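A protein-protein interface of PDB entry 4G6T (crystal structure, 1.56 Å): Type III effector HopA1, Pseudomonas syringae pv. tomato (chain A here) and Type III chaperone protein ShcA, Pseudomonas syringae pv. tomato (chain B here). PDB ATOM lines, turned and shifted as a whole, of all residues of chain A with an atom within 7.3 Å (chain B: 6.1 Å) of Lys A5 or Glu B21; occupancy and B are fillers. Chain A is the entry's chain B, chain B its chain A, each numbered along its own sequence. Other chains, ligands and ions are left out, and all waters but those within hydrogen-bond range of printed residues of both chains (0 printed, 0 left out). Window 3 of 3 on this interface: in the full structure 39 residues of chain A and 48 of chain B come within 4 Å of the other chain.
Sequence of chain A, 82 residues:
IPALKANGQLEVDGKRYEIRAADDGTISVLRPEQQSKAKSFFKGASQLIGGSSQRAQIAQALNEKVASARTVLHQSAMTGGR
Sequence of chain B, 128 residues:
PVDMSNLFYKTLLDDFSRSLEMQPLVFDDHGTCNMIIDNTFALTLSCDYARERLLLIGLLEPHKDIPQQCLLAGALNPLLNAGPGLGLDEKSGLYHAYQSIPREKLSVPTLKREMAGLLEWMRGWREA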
ATOM      1  N   LEU A   4     -20.199 -22.688  -4.695  1.00  0.00           N
ATOM      2  CA  LEU A   4     -18.753 -22.777  -5.101  1.00  0.00           C
ATOM      3  C   LEU A   4     -17.844 -22.918  -3.842  1.00  0.00           C
ATOM      4  O   LEU A   4     -16.936 -22.133  -3.628  1.00  0.00           O
ATOM      5  CB  LEU A   4     -18.396 -21.536  -5.942  1.00  0.00           C
ATOM      6  CG  LEU A   4     -19.516 -20.922  -6.817  1.00  0.00           C
ATOM      7  CD1 LEU A   4     -20.197 -21.947  -7.729  1.00  0.00           C
ATOM      8  CD2 LEU A   4     -20.559 -20.199  -5.962  1.00  0.00           C
ATOM      9  N   LYS A   5     -18.101 -23.950  -3.042  1.00  0.00           N
ATOM     10  CA  LYS A   5     -17.754 -23.957  -1.595  1.00  0.00           C
ATOM     11  C   LYS A   5     -16.253 -24.035  -1.277  1.00  0.00           C
ATOM     12  O   LYS A   5     -15.465 -24.602  -2.035  1.00  0.00           O
ATOM     13  CB  LYS A   5     -18.514 -25.081  -0.864  1.00  0.00           C
ATOM     14  CG  LYS A   5     -18.342 -26.497  -1.414  1.00  0.00           C
ATOM     15  CD  LYS A   5     -19.095 -27.560  -0.607  1.00  0.00           C
ATOM     16  CE  LYS A   5     -18.720 -28.972  -1.067  1.00  0.00           C
ATOM     17  NZ  LYS A   5     -19.619 -30.055  -0.568  1.00  0.00           N
ATOM     18  N   ALA A   6     -15.874 -23.461  -0.141  1.00  0.00           N
ATOM     19  CA  ALA A   6     -14.477 -23.461   0.319  1.00  0.00           C
ATOM     20  C   ALA A   6     -14.161 -24.793   0.992  1.00  0.00           C
ATOM     21  O   ALA A   6     -13.000 -25.176   1.140  1.00  0.00           O
ATOM     22  CB  ALA A   6     -14.265 -22.313   1.294  1.00  0.00           C
ATOM     23  N   ASN A   7     -15.193 -25.509   1.414  1.00  0.00           N
ATOM     24  CA  ASN A   7     -14.997 -26.688   2.238  1.00  0.00           C
ATOM     25  C   ASN A   7     -15.337 -27.956   1.489  1.00  0.00           C
ATOM     26  O   ASN A   7     -16.491 -28.329   1.304  1.00  0.00           O
ATOM     27  CB  ASN A   7     -15.717 -26.570   3.580  1.00  0.00           C
ATOM     28  CG  ASN A   7     -17.191 -26.252   3.436  1.00  0.00           C
ATOM     29  OD1 ASN A   7     -17.562 -25.326   2.717  1.00  0.00           O
ATOM     30  ND2 ASN A   7     -18.034 -27.013   4.119  1.00  0.00           N
ATOM     31  N   GLY A   8     -14.292 -28.632   1.046  1.00  0.00           N
ATOM     32  CA  GLY A   8     -14.448 -29.870   0.334  1.00  0.00           C
ATOM     33  C   GLY A   8     -14.704 -31.021   1.254  1.00  0.00           C
ATOM     34  O   GLY A   8     -14.291 -31.014   2.419  1.00  0.00           O
ATOM     35  N   GLN A   9     -15.315 -32.036   0.706  1.00  0.00           N
ATOM     36  CA  GLN A   9     -15.620 -33.217   1.447  1.00  0.00           C
ATOM     37  C   GLN A   9     -14.895 -34.380   0.777  1.00  0.00           C
ATOM     38  O   GLN A   9     -15.147 -34.752  -0.392  1.00  0.00           O
ATOM     39  CB  GLN A   9     -17.137 -33.422   1.549  1.00  0.00           C
ATOM     40  CG  GLN A   9     -17.876 -32.221   2.119  1.00  0.00           C
ATOM     41  CD  GLN A   9     -17.532 -31.907   3.564  1.00  0.00           C
ATOM     42  OE1 GLN A   9     -17.205 -32.800   4.374  1.00  0.00           O
ATOM     43  NE2 GLN A   9     -17.562 -30.617   3.892  1.00  0.00           N
ATOM     44  N   LEU A  10     -13.891 -34.874   1.491  1.00  0.00           N
ATOM     45  CA  LEU A  10     -13.112 -36.006   1.076  1.00  0.00           C
ATOM     46  C   LEU A  10     -13.781 -37.199   1.675  1.00  0.00           C
ATOM     47  O   LEU A  10     -13.825 -37.303   2.910  1.00  0.00           O
ATOM     48  CB  LEU A  10     -11.665 -35.877   1.585  1.00  0.00           C
ATOM     49  CG  LEU A  10     -10.803 -37.174   1.580  1.00  0.00           C
ATOM     50  CD1 LEU A  10     -10.581 -37.613   0.155  1.00  0.00           C
ATOM     51  CD2 LEU A  10      -9.491 -36.993   2.338  1.00  0.00           C
ATOM     52  N   ILE A  19     -12.034 -30.475   4.079  1.00  0.00           N
ATOM     53  CA  ILE A  19     -10.778 -29.898   3.697  1.00  0.00           C
ATOM     54  C   ILE A  19     -10.930 -28.426   3.424  1.00  0.00           C
ATOM     55  O   ILE A  19     -11.846 -28.035   2.658  1.00  0.00           O
ATOM     56  CB  ILE A  19     -10.331 -30.459   2.335  1.00  0.00           C
ATOM     57  CG1 ILE A  19     -10.398 -31.958   2.283  1.00  0.00           C
ATOM     58  CG2 ILE A  19      -8.963 -29.954   1.973  1.00  0.00           C
ATOM     59  CD1 ILE A  19      -9.632 -32.714   3.321  1.00  0.00           C
ATOM     60  N   ARG A  20     -10.046 -27.609   3.938  1.00  0.00           N
ATOM     61  CA  ARG A  20      -9.968 -26.186   3.591  1.00  0.00           C
ATOM     62  C   ARG A  20      -8.560 -25.802   3.296  1.00  0.00           C
ATOM     63  O   ARG A  20      -7.651 -26.266   3.949  1.00  0.00           O
ATOM     64  CB  ARG A  20     -10.452 -25.323   4.748  1.00  0.00           C
ATOM     65  CG  ARG A  20     -11.880 -25.529   5.097  1.00  0.00           C
ATOM     66  CD  ARG A  20     -12.294 -24.581   6.207  1.00  0.00           C
ATOM     67  NE  ARG A  20     -13.722 -24.744   6.465  1.00  0.00           N
ATOM     68  CZ  ARG A  20     -14.699 -23.991   5.947  1.00  0.00           C
ATOM     69  NH1 ARG A  20     -14.437 -22.966   5.128  1.00  0.00           N
ATOM     70  NH2 ARG A  20     -15.968 -24.269   6.259  1.00  0.00           N
ATOM     71  N   PHE B  16      -8.774 -33.555  -8.073  1.00  0.00           N
ATOM     72  CA  PHE B  16      -9.079 -33.863  -6.658  1.00  0.00           C
ATOM     73  C   PHE B  16     -10.072 -32.853  -6.099  1.00  0.00           C
ATOM     74  O   PHE B  16     -11.081 -33.246  -5.508  1.00  0.00           O
ATOM     75  CB  PHE B  16      -7.742 -33.867  -5.905  1.00  0.00           C
ATOM     76  CG  PHE B  16      -7.830 -34.019  -4.402  1.00  0.00           C
ATOM     77  CD1 PHE B  16      -7.983 -35.263  -3.855  1.00  0.00           C
ATOM     78  CD2 PHE B  16      -7.615 -32.929  -3.586  1.00  0.00           C
ATOM     79  CE1 PHE B  16      -7.988 -35.433  -2.471  1.00  0.00           C
ATOM     80  CE2 PHE B  16      -7.635 -33.077  -2.194  1.00  0.00           C
ATOM     81  CZ  PHE B  16      -7.831 -34.334  -1.661  1.00  0.00           C
ATOM     82  N   SER B  17      -9.837 -31.573  -6.380  1.00  0.00           N
ATOM     83  CA  SER B  17     -10.690 -30.470  -5.920  1.00  0.00           C
ATOM     84  C   SER B  17     -12.078 -30.685  -6.538  1.00  0.00           C
ATOM     85  O   SER B  17     -13.094 -30.541  -5.874  1.00  0.00           O
ATOM     86  CB  SER B  17     -10.109 -29.126  -6.307  1.00  0.00           C
ATOM     87  OG  SER B  17      -8.823 -28.854  -5.766  1.00  0.00           O
ATOM     88  N   ARG B  18     -12.130 -31.062  -7.802  1.00  0.00           N
ATOM     89  CA  ARG B  18     -13.444 -31.269  -8.465  1.00  0.00           C
ATOM     90  C   ARG B  18     -14.199 -32.409  -7.814  1.00  0.00           C
ATOM     91  O   ARG B  18     -15.433 -32.369  -7.667  1.00  0.00           O
ATOM     92  CB  ARG B  18     -13.248 -31.582  -9.947  1.00  0.00           C
ATOM     93  CG  ARG B  18     -12.936 -30.371 -10.807  1.00  0.00           C
ATOM     94  CD  ARG B  18     -12.657 -30.800 -12.239  1.00  0.00           C
ATOM     95  NE  ARG B  18     -12.213 -29.674 -13.041  1.00  0.00           N
ATOM     96  CZ  ARG B  18     -12.086 -29.662 -14.371  1.00  0.00           C
ATOM     97  NH1 ARG B  18     -12.359 -30.722 -15.141  1.00  0.00           N
ATOM     98  NH2 ARG B  18     -11.687 -28.547 -14.944  1.00  0.00           N
ATOM     99  N   SER B  19     -13.468 -33.441  -7.427  1.00  0.00           N
ATOM    100  CA  SER B  19     -14.061 -34.591  -6.746  1.00  0.00           C
ATOM    101  C   SER B  19     -14.611 -34.166  -5.367  1.00  0.00           C
ATOM    102  O   SER B  19     -15.660 -34.631  -4.953  1.00  0.00           O
ATOM    103  CB  SER B  19     -13.023 -35.688  -6.538  1.00  0.00           C
ATOM    104  OG  SER B  19     -13.663 -36.916  -6.252  1.00  0.00           O
ATOM    105  N   LEU B  20     -13.848 -33.336  -4.672  1.00  0.00           N
ATOM    106  CA  LEU B  20     -14.159 -32.835  -3.317  1.00  0.00           C
ATOM    107  C   LEU B  20     -15.295 -31.789  -3.391  1.00  0.00           C
ATOM    108  O   LEU B  20     -15.758 -31.281  -2.365  1.00  0.00           O
ATOM    109  CB  LEU B  20     -12.905 -32.225  -2.670  1.00  0.00           C
ATOM    110  CG  LEU B  20     -12.159 -33.171  -1.698  1.00  0.00           C
ATOM    111  CD1 LEU B  20     -11.815 -34.523  -2.306  1.00  0.00           C
ATOM    112  CD2 LEU B  20     -10.931 -32.407  -1.222  1.00  0.00           C
ATOM    113  N   GLU B  21     -15.707 -31.468  -4.624  1.00  0.00           N
ATOM    114  CA  GLU B  21     -16.656 -30.398  -4.973  1.00  0.00           C
ATOM    115  C   GLU B  21     -16.355 -29.078  -4.285  1.00  0.00           C
ATOM    116  O   GLU B  21     -17.181 -28.545  -3.562  1.00  0.00           O
ATOM    117  CB  GLU B  21     -18.098 -30.852  -4.669  1.00  0.00           C
ATOM    118  CG  GLU B  21     -18.488 -32.102  -5.442  1.00  0.00           C
ATOM    119  CD  GLU B  21     -19.861 -32.635  -5.071  1.00  0.00           C
ATOM    120  OE1 GLU B  21     -20.400 -32.271  -4.000  1.00  0.00           O
ATOM    121  OE2 GLU B  21     -20.398 -33.430  -5.863  1.00  0.00           O
ATOM    122  N   MET B  22     -15.167 -28.544  -4.507  1.00  0.00           N
ATOM    123  CA  MET B  22     -14.718 -27.363  -3.816  1.00  0.00           C
ATOM    124  C   MET B  22     -13.960 -26.427  -4.717  1.00  0.00           C
ATOM    125  O   MET B  22     -13.439 -26.790  -5.805  1.00  0.00           O
ATOM    126  CB  MET B  22     -13.847 -27.705  -2.581  1.00  0.00           C
ATOM    127  CG  MET B  22     -12.464 -28.209  -2.956  1.00  0.00           C
ATOM    128  SD  MET B  22     -11.468 -28.821  -1.555  1.00  0.00           S
ATOM    129  CE  MET B  22     -10.854 -27.332  -0.876  1.00  0.00           C
ATOM    130  N   GLN B  23     -13.857 -25.212  -4.256  1.00  0.00           N
ATOM    131  CA  GLN B  23     -13.058 -24.240  -4.903  1.00  0.00           C
ATOM    132  C   GLN B  23     -11.667 -24.854  -5.116  1.00  0.00           C
ATOM    133  O   GLN B  23     -11.157 -25.440  -4.190  1.00  0.00           O
ATOM    134  CB  GLN B  23     -12.921 -23.090  -3.939  1.00  0.00           C
ATOM    135  CG  GLN B  23     -11.986 -22.006  -4.357  1.00  0.00           C
ATOM    136  CD  GLN B  23     -11.866 -20.968  -3.262  1.00  0.00           C
ATOM    137  OE1 GLN B  23     -12.841 -20.668  -2.554  1.00  0.00           O
ATOM    138  NE2 GLN B  23     -10.665 -20.429  -3.095  1.00  0.00           N
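O of Lys A5 lies within hydrogen-bond range of N of Gln B23.
O of Leu B20 sits at hydrogen-bond distance from N of Gln A9 (3.2 Å).
O of Gly A8 lies within hydrogen-bond range of N of Ile A19 (2.9 Å).
N of Met B22 is in hydrogen-bond range of O of Ser B17 (3.2 Å).
Lys A5 touches Leu B20.
Lys A5 touches Glu B21.
CA of Met B22 touches O of Lys A5 (3.4 Å).
CE of Met B22 touches O of Ala A6, at 3.6 Å.
CA of Gly A8 touches O of Leu B20, at 3.3 Å.
Met B22 touches Gly A8.
CA of Leu A10 touches CD1 of Leu B20, 3.9 Å away.
Leu B20 touches Ile A19.
O of Ile A19 touches CE of Met B22, 3.7 Å away.
Lys A5 touches just these residues of chain B: Leu B20 (3.97 Å), Glu B21 (3.0 Å), Met B22 (3.4 Å) and Gln B23 (2.8 Å).
Glu B21 touches just one residue of chain A: Lys A5 (3.0 Å).
Of the printed residues of chain A, Met B22 touches Lys A5, Ala A6, Gly A8 and Ile A19.
Of the printed residues of chain B, Gly A8 touches Leu B20 (3.3 Å) and Met B22 (3.7 Å).
Of the printed residues of chain B, Leu A10 touches Leu B20.
Of the printed residues of chain B, Gln A9 touches Leu B20.
Ser B17 touches none of the printed residues of chain A.
The nearest printed residue of chain B that does not touch Lys A5 is Ser B17 (7.5 Å).
The nearest printed residue of chain A that does not touch Glu B21 is Asn A7 (4.9 Å).
Of the 9 printed residues of chain A, 6 touch a printed residue of chain B.
Hydrophobic or aromatic side chains of chain A that line the printed part of chain B: Ile A19.
Along chain A the printed residues that touch a printed residue of chain B span positions 5 to 19.
Among the printed residues, no Asp or Glu carboxylate lies within 4 Å of a Lys or Arg side-chain nitrogen of the other chain.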
